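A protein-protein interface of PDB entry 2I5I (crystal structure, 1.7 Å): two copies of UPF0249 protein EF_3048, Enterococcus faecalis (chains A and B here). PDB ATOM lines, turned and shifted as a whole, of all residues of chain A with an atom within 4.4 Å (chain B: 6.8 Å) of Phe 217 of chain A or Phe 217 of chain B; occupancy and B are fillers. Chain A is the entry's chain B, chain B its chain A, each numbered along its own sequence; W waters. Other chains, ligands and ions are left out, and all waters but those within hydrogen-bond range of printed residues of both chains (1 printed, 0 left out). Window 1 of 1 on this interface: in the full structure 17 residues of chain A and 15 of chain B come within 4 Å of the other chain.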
ATOM      1  N   PRO A  18      14.638 -25.685   8.898  1.00  0.00           N
ATOM      2  CA  PRO A  18      13.843 -25.965  10.110  1.00  0.00           C
ATOM      3  C   PRO A  18      12.344 -25.870   9.872  1.00  0.00           C
ATOM      4  O   PRO A  18      11.534 -26.642  10.375  1.00  0.00           O
ATOM      5  CB  PRO A  18      14.321 -24.868  11.072  1.00  0.00           C
ATOM      6  CG  PRO A  18      15.710 -24.578  10.603  1.00  0.00           C
ATOM      7  CD  PRO A  18      15.625 -24.612   9.097  1.00  0.00           C
ATOM      8  N   ALA A  19      11.856 -24.908   9.092  1.00  0.00           N
ATOM      9  CA  ALA A  19      10.433 -24.774   8.835  1.00  0.00           C
ATOM     10  C   ALA A  19       9.837 -25.847   7.926  1.00  0.00           C
ATOM     11  O   ALA A  19       8.706 -26.284   8.049  1.00  0.00           O
ATOM     12  CB  ALA A  19      10.152 -23.417   8.196  1.00  0.00           C
ATOM     13  N   VAL A  20      10.639 -26.271   6.957  1.00  0.00           N
ATOM     14  CA  VAL A  20      10.255 -27.389   6.114  1.00  0.00           C
ATOM     15  C   VAL A  20      10.048 -28.608   7.002  1.00  0.00           C
ATOM     16  O   VAL A  20       8.987 -29.231   6.971  1.00  0.00           O
ATOM     17  CB  VAL A  20      11.314 -27.665   5.031  1.00  0.00           C
ATOM     18  CG1 VAL A  20      11.023 -29.008   4.374  1.00  0.00           C
ATOM     19  CG2 VAL A  20      11.319 -26.539   4.005  1.00  0.00           C
ATOM     20  N   GLN A  22       9.377 -28.811  10.070  1.00  0.00           N
ATOM     21  CA  GLN A  22       8.222 -28.780  10.965  1.00  0.00           C
ATOM     22  C   GLN A  22       6.897 -28.856  10.219  1.00  0.00           C
ATOM     23  O   GLN A  22       5.928 -29.438  10.687  1.00  0.00           O
ATOM     24  CB  GLN A  22       8.285 -27.506  11.805  1.00  0.00           C
ATOM     25  CG  GLN A  22       9.294 -27.506  12.933  1.00  0.00           C
ATOM     26  CD  GLN A  22       9.253 -28.761  13.789  1.00  0.00           C
ATOM     27  OE1 GLN A  22       8.180 -29.167  14.237  1.00  0.00           O
ATOM     28  NE2 GLN A  22      10.404 -29.379  14.001  1.00  0.00           N
ATOM     29  N   GLY A  23       6.862 -28.264   9.028  1.00  0.00           N
ATOM     30  CA  GLY A  23       5.661 -28.357   8.203  1.00  0.00           C
ATOM     31  C   GLY A  23       5.409 -29.813   7.839  1.00  0.00           C
ATOM     32  O   GLY A  23       4.268 -30.252   7.814  1.00  0.00           O
ATOM     33  N   GLU A  26       3.921 -31.625  10.742  1.00  0.00           N
ATOM     34  CA  GLU A  26       2.525 -31.211  10.912  1.00  0.00           C
ATOM     35  C   GLU A  26       1.640 -32.009   9.959  1.00  0.00           C
ATOM     36  O   GLU A  26       0.594 -32.563  10.313  1.00  0.00           O
ATOM     37  CB  GLU A  26       2.380 -29.706  10.702  1.00  0.00           C
ATOM     38  CG  GLU A  26       0.949 -29.200  10.822  1.00  0.00           C
ATOM     39  CD  GLU A  26       0.401 -29.114  12.225  1.00  0.00           C
ATOM     40  OE1 GLU A  26       1.160 -29.319  13.199  1.00  0.00           O
ATOM     41  OE2 GLU A  26      -0.815 -28.842  12.379  1.00  0.00           O
ATOM     42  N   ALA A 216       5.566 -27.776   3.747  1.00  0.00           N
ATOM     43  CA  ALA A 216       6.502 -27.013   4.551  1.00  0.00           C
ATOM     44  C   ALA A 216       5.766 -25.865   5.259  1.00  0.00           C
ATOM     45  O   ALA A 216       4.722 -25.465   4.750  1.00  0.00           O
ATOM     46  CB  ALA A 216       7.647 -26.426   3.729  1.00  0.00           C
ATOM     47  N   PHE A 217       6.325 -25.408   6.371  1.00  0.00           N
ATOM     48  CA  PHE A 217       6.137 -24.050   6.859  1.00  0.00           C
ATOM     49  C   PHE A 217       7.231 -23.208   6.187  1.00  0.00           C
ATOM     50  O   PHE A 217       8.228 -23.758   5.723  1.00  0.00           O
ATOM     51  CB  PHE A 217       6.243 -23.912   8.370  1.00  0.00           C
ATOM     52  CG  PHE A 217       5.201 -24.732   9.120  1.00  0.00           C
ATOM     53  CD1 PHE A 217       3.946 -25.026   8.607  1.00  0.00           C
ATOM     54  CD2 PHE A 217       5.496 -25.222  10.367  1.00  0.00           C
ATOM     55  CE1 PHE A 217       3.064 -25.804   9.350  1.00  0.00           C
ATOM     56  CE2 PHE A 217       4.619 -25.990  11.111  1.00  0.00           C
ATOM     57  CZ  PHE A 217       3.358 -26.281  10.607  1.00  0.00           C
ATOM     58  N   ILE A 218       7.024 -21.906   6.155  1.00  0.00           N
ATOM     59  CA  ILE A 218       7.925 -20.970   5.510  1.00  0.00           C
ATOM     60  C   ILE A 218       8.867 -20.320   6.521  1.00  0.00           C
ATOM     61  O   ILE A 218       8.404 -19.799   7.538  1.00  0.00           O
ATOM     62  CB  ILE A 218       7.181 -19.840   4.769  1.00  0.00           C
ATOM     63  CG1 ILE A 218       6.124 -20.296   3.766  1.00  0.00           C
ATOM     64  CG2 ILE A 218       8.212 -18.908   4.130  1.00  0.00           C
ATOM     65  CD1 ILE A 218       6.555 -21.470   2.907  1.00  0.00           C
ATOM     66  N   ASP A 219      10.156 -20.380   6.221  1.00  0.00           N
ATOM     67  CA  ASP A 219      11.151 -19.576   6.942  1.00  0.00           C
ATOM     68  C   ASP A 219      11.953 -18.821   5.884  1.00  0.00           C
ATOM     69  O   ASP A 219      11.834 -19.082   4.685  1.00  0.00           O
ATOM     70  CB  ASP A 219      12.034 -20.365   7.881  1.00  0.00           C
ATOM     71  CG  ASP A 219      12.746 -21.595   7.359  1.00  0.00           C
ATOM     72  OD1 ASP A 219      12.679 -21.876   6.136  1.00  0.00           O
ATOM     73  OD2 ASP A 219      13.353 -22.285   8.211  1.00  0.00           O
ATOM     74  N   LEU A 222      14.102 -21.208   3.592  1.00  0.00           N
ATOM     75  CA  LEU A 222      13.412 -21.781   2.431  1.00  0.00           C
ATOM     76  C   LEU A 222      13.299 -20.745   1.322  1.00  0.00           C
ATOM     77  O   LEU A 222      13.620 -21.022   0.163  1.00  0.00           O
ATOM     78  CB  LEU A 222      12.034 -22.293   2.850  1.00  0.00           C
ATOM     79  CG  LEU A 222      11.114 -22.801   1.738  1.00  0.00           C
ATOM     80  CD1 LEU A 222      11.802 -23.891   0.924  1.00  0.00           C
ATOM     81  CD2 LEU A 222       9.795 -23.282   2.316  1.00  0.00           C
ATOM     82  N   ILE A 233       2.857 -24.312   1.782  1.00  0.00           N
ATOM     83  CA  ILE A 233       1.939 -24.277   2.938  1.00  0.00           C
ATOM     84  C   ILE A 233       0.555 -24.732   2.528  1.00  0.00           C
ATOM     85  O   ILE A 233      -0.268 -25.251   3.285  1.00  0.00           O
ATOM     86  CB  ILE A 233       1.883 -22.876   3.589  1.00  0.00           C
ATOM     87  CG1 ILE A 233       1.372 -21.763   2.687  1.00  0.00           C
ATOM     88  CG2 ILE A 233       3.258 -22.522   4.135  1.00  0.00           C
ATOM     89  CD1 ILE A 233       1.559 -20.348   3.186  1.00  0.00           C
ATOM     90  N   THR B  17      -0.914 -20.428  16.163  1.00  0.00           N
ATOM     91  CA  THR B  17      -1.055 -21.474  15.147  1.00  0.00           C
ATOM     92  C   THR B  17       0.157 -22.405  15.220  1.00  0.00           C
ATOM     93  O   THR B  17       1.204 -22.026  15.758  1.00  0.00           O
ATOM     94  CB  THR B  17      -1.279 -20.935  13.733  1.00  0.00           C
ATOM     95  OG1 THR B  17      -0.073 -20.977  12.972  1.00  0.00           O
ATOM     96  CG2 THR B  17      -1.621 -19.442  13.615  1.00  0.00           C
ATOM     97  N   PRO B  18       0.055 -23.623  14.708  1.00  0.00           N
ATOM     98  CA  PRO B  18       1.211 -24.540  14.739  1.00  0.00           C
ATOM     99  C   PRO B  18       2.519 -23.960  14.231  1.00  0.00           C
ATOM    100  O   PRO B  18       3.570 -24.194  14.818  1.00  0.00           O
ATOM    101  CB  PRO B  18       0.727 -25.687  13.818  1.00  0.00           C
ATOM    102  CG  PRO B  18      -0.745 -25.716  14.117  1.00  0.00           C
ATOM    103  CD  PRO B  18      -1.112 -24.239  14.088  1.00  0.00           C
ATOM    104  N   ALA B  19       2.555 -23.196  13.141  1.00  0.00           N
ATOM    105  CA  ALA B  19       3.777 -22.621  12.633  1.00  0.00           C
ATOM    106  C   ALA B  19       4.287 -21.424  13.439  1.00  0.00           C
ATOM    107  O   ALA B  19       5.484 -21.185  13.501  1.00  0.00           O
ATOM    108  CB  ALA B  19       3.610 -22.144  11.187  1.00  0.00           C
ATOM    109  N   VAL B  20       3.366 -20.669  14.035  1.00  0.00           N
ATOM    110  CA  VAL B  20       3.798 -19.608  14.939  1.00  0.00           C
ATOM    111  C   VAL B  20       4.537 -20.279  16.099  1.00  0.00           C
ATOM    112  O   VAL B  20       5.675 -19.911  16.357  1.00  0.00           O
ATOM    113  CB  VAL B  20       2.632 -18.748  15.444  1.00  0.00           C
ATOM    114  CG1 VAL B  20       3.131 -17.827  16.561  1.00  0.00           C
ATOM    115  CG2 VAL B  20       2.016 -17.924  14.328  1.00  0.00           C
ATOM    116  N   THR B  21       3.925 -21.262  16.747  1.00  0.00           N
ATOM    117  CA  THR B  21       4.542 -21.988  17.860  1.00  0.00           C
ATOM    118  C   THR B  21       5.936 -22.477  17.490  1.00  0.00           C
ATOM    119  O   THR B  21       6.923 -22.346  18.216  1.00  0.00           O
ATOM    120  CB  THR B  21       3.649 -23.148  18.291  1.00  0.00           C
ATOM    121  OG1 THR B  21       2.449 -22.574  18.892  1.00  0.00           O
ATOM    122  CG2 THR B  21       4.274 -24.063  19.330  1.00  0.00           C
ATOM    123  N   GLN B  22       6.080 -23.070  16.294  1.00  0.00           N
ATOM    124  CA  GLN B  22       7.426 -23.596  15.989  1.00  0.00           C
ATOM    125  C   GLN B  22       8.408 -22.494  15.613  1.00  0.00           C
ATOM    126  O   GLN B  22       9.612 -22.588  15.851  1.00  0.00           O
ATOM    127  CB  GLN B  22       7.345 -24.645  14.883  1.00  0.00           C
ATOM    128  CG  GLN B  22       6.570 -25.902  15.258  1.00  0.00           C
ATOM    129  CD  GLN B  22       7.206 -26.636  16.421  1.00  0.00           C
ATOM    130  OE1 GLN B  22       8.421 -26.739  16.503  1.00  0.00           O
ATOM    131  NE2 GLN B  22       6.420 -27.211  17.330  1.00  0.00           N
ATOM    132  N   GLY B  23       7.922 -21.403  15.027  1.00  0.00           N
ATOM    133  CA  GLY B  23       8.791 -20.265  14.785  1.00  0.00           C
ATOM    134  C   GLY B  23       9.297 -19.656  16.081  1.00  0.00           C
ATOM    135  O   GLY B  23      10.463 -19.293  16.175  1.00  0.00           O
ATOM    136  N   ILE B  24       8.418 -19.561  17.084  1.00  0.00           N
ATOM    137  CA  ILE B  24       8.906 -19.086  18.386  1.00  0.00           C
ATOM    138  C   ILE B  24       9.929 -20.022  18.988  1.00  0.00           C
ATOM    139  O   ILE B  24      10.978 -19.602  19.481  1.00  0.00           O
ATOM    140  CB  ILE B  24       7.721 -18.880  19.346  1.00  0.00           C
ATOM    141  CG1 ILE B  24       6.864 -17.679  18.916  1.00  0.00           C
ATOM    142  CG2 ILE B  24       8.172 -18.702  20.776  1.00  0.00           C
ATOM    143  CD1 ILE B  24       5.471 -17.679  19.482  1.00  0.00           C
ATOM    144  N   ILE B  25       9.667 -21.339  18.948  1.00  0.00           N
ATOM    145  CA  ILE B  25      10.644 -22.279  19.498  1.00  0.00           C
ATOM    146  C   ILE B  25      11.995 -22.131  18.826  1.00  0.00           C
ATOM    147  O   ILE B  25      13.026 -22.188  19.502  1.00  0.00           O
ATOM    148  CB  ILE B  25      10.083 -23.717  19.411  1.00  0.00           C
ATOM    149  CG1 ILE B  25       8.949 -23.954  20.400  1.00  0.00           C
ATOM    150  CG2 ILE B  25      11.187 -24.757  19.589  1.00  0.00           C
ATOM    151  CD1 ILE B  25       8.188 -25.265  20.322  1.00  0.00           C
ATOM    152  N   GLU B  26      12.030 -21.916  17.514  1.00  0.00           N
ATOM    153  CA  GLU B  26      13.279 -21.701  16.784  1.00  0.00           C
ATOM    154  C   GLU B  26      14.069 -20.487  17.273  1.00  0.00           C
ATOM    155  O   GLU B  26      15.272 -20.494  17.474  1.00  0.00           O
ATOM    156  CB  GLU B  26      12.935 -21.546  15.300  1.00  0.00           C
ATOM    157  CG  GLU B  26      14.136 -21.409  14.392  1.00  0.00           C
ATOM    158  CD  GLU B  26      15.007 -22.637  14.227  1.00  0.00           C
ATOM    159  OE1 GLU B  26      14.620 -23.756  14.628  1.00  0.00           O
ATOM    160  OE2 GLU B  26      16.127 -22.476  13.674  1.00  0.00           O
ATOM    161  N   ALA B  27      13.318 -19.399  17.415  1.00  0.00           N
ATOM    162  CA  ALA B  27      13.854 -18.121  17.858  1.00  0.00           C
ATOM    163  C   ALA B  27      14.416 -18.216  19.266  1.00  0.00           C
ATOM    164  O   ALA B  27      15.346 -17.495  19.617  1.00  0.00           O
ATOM    165  CB  ALA B  27      12.722 -17.089  17.766  1.00  0.00           C
ATOM    166  N   PRO B 215       7.947 -13.496  16.327  1.00  0.00           N
ATOM    167  CA  PRO B 215       8.532 -14.484  15.407  1.00  0.00           C
ATOM    168  C   PRO B 215       7.489 -15.567  15.120  1.00  0.00           C
ATOM    169  O   PRO B 215       6.629 -15.872  15.939  1.00  0.00           O
ATOM    170  CB  PRO B 215       9.691 -15.081  16.172  1.00  0.00           C
ATOM    171  CG  PRO B 215       9.540 -14.670  17.598  1.00  0.00           C
ATOM    172  CD  PRO B 215       8.566 -13.532  17.651  1.00  0.00           C
ATOM    173  N   ALA B 216       7.581 -16.164  13.945  1.00  0.00           N
ATOM    174  CA  ALA B 216       6.768 -17.265  13.486  1.00  0.00           C
ATOM    175  C   ALA B 216       7.359 -17.831  12.188  1.00  0.00           C
ATOM    176  O   ALA B 216       8.084 -17.115  11.516  1.00  0.00           O
ATOM    177  CB  ALA B 216       5.335 -16.858  13.207  1.00  0.00           C
ATOM    178  N   PHE B 217       7.020 -19.085  11.929  1.00  0.00           N
ATOM    179  CA  PHE B 217       7.021 -19.657  10.603  1.00  0.00           C
ATOM    180  C   PHE B 217       5.623 -19.390  10.050  1.00  0.00           C
ATOM    181  O   PHE B 217       4.689 -19.168  10.822  1.00  0.00           O
ATOM    182  CB  PHE B 217       7.359 -21.144  10.584  1.00  0.00           C
ATOM    183  CG  PHE B 217       8.726 -21.496  11.131  1.00  0.00           C
ATOM    184  CD1 PHE B 217       9.839 -20.678  11.031  1.00  0.00           C
ATOM    185  CD2 PHE B 217       8.932 -22.712  11.781  1.00  0.00           C
ATOM    186  CE1 PHE B 217      11.076 -21.089  11.527  1.00  0.00           C
ATOM    187  CE2 PHE B 217      10.134 -23.129  12.295  1.00  0.00           C
ATOM    188  CZ  PHE B 217      11.222 -22.286  12.186  1.00  0.00           C
ATOM    189  N   ILE B 218       5.475 -19.424   8.742  1.00  0.00           N
ATOM    190  CA  ILE B 218       4.170 -19.199   8.122  1.00  0.00           C
ATOM    191  C   ILE B 218       3.477 -20.525   7.797  1.00  0.00           C
ATOM    192  O   ILE B 218       4.103 -21.414   7.198  1.00  0.00           O
ATOM    193  CB  ILE B 218       4.265 -18.359   6.837  1.00  0.00           C
ATOM    194  CG1 ILE B 218       4.981 -17.019   6.959  1.00  0.00           C
ATOM    195  CG2 ILE B 218       2.870 -18.116   6.272  1.00  0.00           C
ATOM    196  CD1 ILE B 218       4.880 -16.359   8.309  1.00  0.00           C
ATOM    197  N   ASP B 219       2.213 -20.604   8.190  1.00  0.00           N
ATOM    198  CA  ASP B 219       1.291 -21.669   7.783  1.00  0.00           C
ATOM    199  C   ASP B 219       0.043 -20.992   7.221  1.00  0.00           C
ATOM    200  O   ASP B 219      -0.113 -19.763   7.279  1.00  0.00           O
ATOM    201  CB  ASP B 219       0.945 -22.679   8.846  1.00  0.00           C
ATOM    202  CG  ASP B 219       0.464 -22.217  10.206  1.00  0.00           C
ATOM    203  OD1 ASP B 219       0.248 -21.012  10.464  1.00  0.00           O
ATOM    204  OD2 ASP B 219       0.315 -23.095  11.086  1.00  0.00           O
ATOM    205  N   THR B 220      -0.851 -21.756   6.616  1.00  0.00           N
ATOM    206  CA  THR B 220      -2.058 -21.099   6.111  1.00  0.00           C
ATOM    207  C   THR B 220      -2.894 -20.577   7.281  1.00  0.00           C
ATOM    208  O   THR B 220      -3.602 -19.595   7.113  1.00  0.00           O
ATOM    209  CB  THR B 220      -2.942 -22.038   5.281  1.00  0.00           C
ATOM    210  OG1 THR B 220      -3.246 -23.199   6.073  1.00  0.00           O
ATOM    211  CG2 THR B 220      -2.204 -22.542   4.051  1.00  0.00           C
ATOM    212  N   ILE B 221      -2.811 -21.257   8.422  1.00  0.00           N
ATOM    213  CA  ILE B 221      -3.624 -20.822   9.569  1.00  0.00           C
ATOM    214  C   ILE B 221      -3.215 -19.401   9.936  1.00  0.00           C
ATOM    215  O   ILE B 221      -4.069 -18.533  10.098  1.00  0.00           O
ATOM    216  CB  ILE B 221      -3.522 -21.780  10.753  1.00  0.00           C
ATOM    217  CG1 ILE B 221      -3.863 -23.231  10.369  1.00  0.00           C
ATOM    218  CG2 ILE B 221      -4.394 -21.364  11.927  1.00  0.00           C
ATOM    219  CD1 ILE B 221      -2.902 -24.184  11.028  1.00  0.00           C
ATOM    220  N   LEU B 222      -1.922 -19.107  10.044  1.00  0.00           N
ATOM    221  CA  LEU B 222      -1.527 -17.724  10.310  1.00  0.00           C
ATOM    222  C   LEU B 222      -2.015 -16.789   9.216  1.00  0.00           C
ATOM    223  O   LEU B 222      -2.561 -15.711   9.470  1.00  0.00           O
ATOM    224  CB  LEU B 222      -0.007 -17.631  10.456  1.00  0.00           C
ATOM    225  CG  LEU B 222       0.562 -16.219  10.594  1.00  0.00           C
ATOM    226  CD1 LEU B 222      -0.021 -15.502  11.797  1.00  0.00           C
ATOM    227  CD2 LEU B 222       2.082 -16.284  10.670  1.00  0.00           C
ATOM    228  N   CYS B 229       1.753 -11.044   9.008  1.00  0.00           N
ATOM    229  CA  CYS B 229       2.094 -12.424   8.637  1.00  0.00           C
ATOM    230  C   CYS B 229       3.523 -12.556   8.154  1.00  0.00           C
ATOM    231  O   CYS B 229       4.420 -12.979   8.886  1.00  0.00           O
ATOM    232  CB  CYS B 229       1.089 -12.874   7.571  1.00  0.00           C
ATOM    233  SG  CYS B 229       1.254 -14.610   7.088  1.00  0.00           S
ATOM    234  N   ARG B 232       6.918 -11.845  10.148  1.00  0.00           N
ATOM    235  CA  ARG B 232       7.272 -12.661  11.315  1.00  0.00           C
ATOM    236  C   ARG B 232       8.433 -13.592  10.991  1.00  0.00           C
ATOM    237  O   ARG B 232       9.226 -13.947  11.866  1.00  0.00           O
ATOM    238  CB  ARG B 232       6.078 -13.450  11.809  1.00  0.00           C
ATOM    239  CG  ARG B 232       4.809 -12.692  12.145  1.00  0.00           C
ATOM    240  CD  ARG B 232       3.984 -13.516  13.147  1.00  0.00           C
ATOM    241  NE  ARG B 232       2.701 -12.872  13.358  1.00  0.00           N
ATOM    242  CZ  ARG B 232       1.958 -12.830  14.437  1.00  0.00           C
ATOM    243  NH1 ARG B 232       2.287 -13.418  15.566  1.00  0.00           N
ATOM    244  NH2 ARG B 232       0.811 -12.161  14.372  1.00  0.00           N
ATOM    245  N   ILE B 233       8.590 -13.999   9.714  1.00  0.00           N
ATOM    246  CA  ILE B 233       9.758 -14.845   9.442  1.00  0.00           C
ATOM    247  C   ILE B 233      11.036 -14.034   9.495  1.00  0.00           C
ATOM    248  O   ILE B 233      12.097 -14.559   9.869  1.00  0.00           O
ATOM    249  CB  ILE B 233       9.628 -15.585   8.098  1.00  0.00           C
ATOM    250  CG1 ILE B 233       9.454 -14.729   6.834  1.00  0.00           C
ATOM    251  CG2 ILE B 233       8.489 -16.602   8.160  1.00  0.00           C
ATOM    252  CD1 ILE B 233       9.718 -15.560   5.576  1.00  0.00           C
ATOM    253  N   VAL B 236      12.324 -13.958  12.958  1.00  0.00           N
ATOM    254  CA  VAL B 236      13.090 -15.146  13.324  1.00  0.00           C
ATOM    255  C   VAL B 236      14.530 -14.985  12.857  1.00  0.00           C
ATOM    256  O   VAL B 236      15.494 -15.274  13.570  1.00  0.00           O
ATOM    257  CB  VAL B 236      12.539 -16.441  12.715  1.00  0.00           C
ATOM    258  CG1 VAL B 236      13.429 -17.603  13.152  1.00  0.00           C
ATOM    259  CG2 VAL B 236      11.103 -16.692  13.134  1.00  0.00           C
HETATM  260  O   HOH W   1       0.004 -24.422   5.949  1.00  0.00           O
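N of Ile 218 of chain A is in hydrogen-bond range of O of Ile 218 of chain B.
The side-chain amide oxygen of Gln 22 of chain B sits close to the side-chain amide oxygen of Gln 22 of chain A (3.3 Å).
The backbone carbonyl oxygen (O) of Ala 19 of chain B sits at hydrogen-bond distance from the backbone NH (N) of Phe 217 of chain B, 3.0 Å away.
OD2 of Asp 219 of chain B sits at hydrogen-bond distance from N of Ala 19 of chain B, at 3.0 Å.
OG1 of Thr 17 of chain B is in hydrogen-bond range of OD1 of Asp 219 of chain B (2.5 Å).
The side-chain carboxylate of Asp 219 of chain A lies within hydrogen-bond range of the backbone NH of Leu 222 of chain A (3.0 Å).
The backbone carbonyl oxygen of Ala 19 of chain A is in hydrogen-bond range of the backbone NH of Phe 217 of chain A, 3.0 Å away.
OG1 of Thr 17 of chain B sits close to N of Ala 19 of chain B (3.4 Å).
CB of Pro 18 of chain A touches OE1 of Glu 26 of chain B, at 3.7 Å.
CB of Ala 19 of chain A touches CG of Phe 217 of chain B, 3.8 Å away.
CG of Pro 18 of chain B touches OE2 of Glu 26 of chain A, 3.6 Å away.
CG of Phe 217 of chain A touches CB of Ala 19 of chain B, 3.7 Å away.
CB of Phe 217 of chain B touches CB of Phe 217 of chain A (3.7 Å).
Phe 217 of chain A touches Asp 219 of chain B.
Ile 233 of chain B touches Ile 218 of chain A (CG2 to O, 3.3 Å).
CD1 of Ile 233 of chain B touches C of Asp 219 of chain A, 3.97 Å away.
Ile 233 of chain A touches Ile 218 of chain B.
Thr 220 of chain B touches Ile 233 of chain A (CG2 to O, 3.4 Å).
Of the printed residues of chain B, Pro 18 of chain A touches Glu 26.
Printed residues of chain A within 4 Å of Asp 219 of chain B: Phe 217.
Printed residues of chain A within 4 Å of Ile 233 of chain B: Ile 218 and Asp 219.
The nearest residue of chain B that does not touch Phe 217 of chain A is Pro 18 of chain B (4.2 Å).
The nearest residue of chain A that does not touch Phe 217 of chain B is Pro 18 of chain A (4.2 Å).
The nearest printed residue of chain B that does not touch Glu 26 of chain A is Ile 221 of chain B (5.3 Å).
Of the 23 printed residues of chain B, 9 touch a printed residue of chain A.
Hydrophobic or aromatic side chains of chain A that line the printed part of chain B: Pro 18, Ala 19, Phe 217, Ile 218 and Ile 233.
Among the printed residues, no Asp or Glu carboxylate lies within 4 Å of a Lys or Arg side-chain nitrogen of the other chain.
Ala 19 of chain A touches Phe 217 of chain B, and with the chains exchanged Phe 217 of chain A touches Ala 19 of chain B.
Gln 22 of chain A touches its own counterpart, Gln 22 of chain B.
Phe 217 of chain A touches Ile 218 of chain B, and with the chains exchanged Ile 218 of chain A touches Phe 217 of chain B.
Asp 219 of chain A touches Ile 233 of chain B, but with the chains exchanged Ile 233 of chain A does not touch Asp 219 of chain B (4.2 Å).
Of the 15 pairs that touch across the chains among the printed residues, 13 have their exchanged pair printed and touching as well.
Water W1 bridges O of Ile 233 of chain A and N of Thr 220 of chain B.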
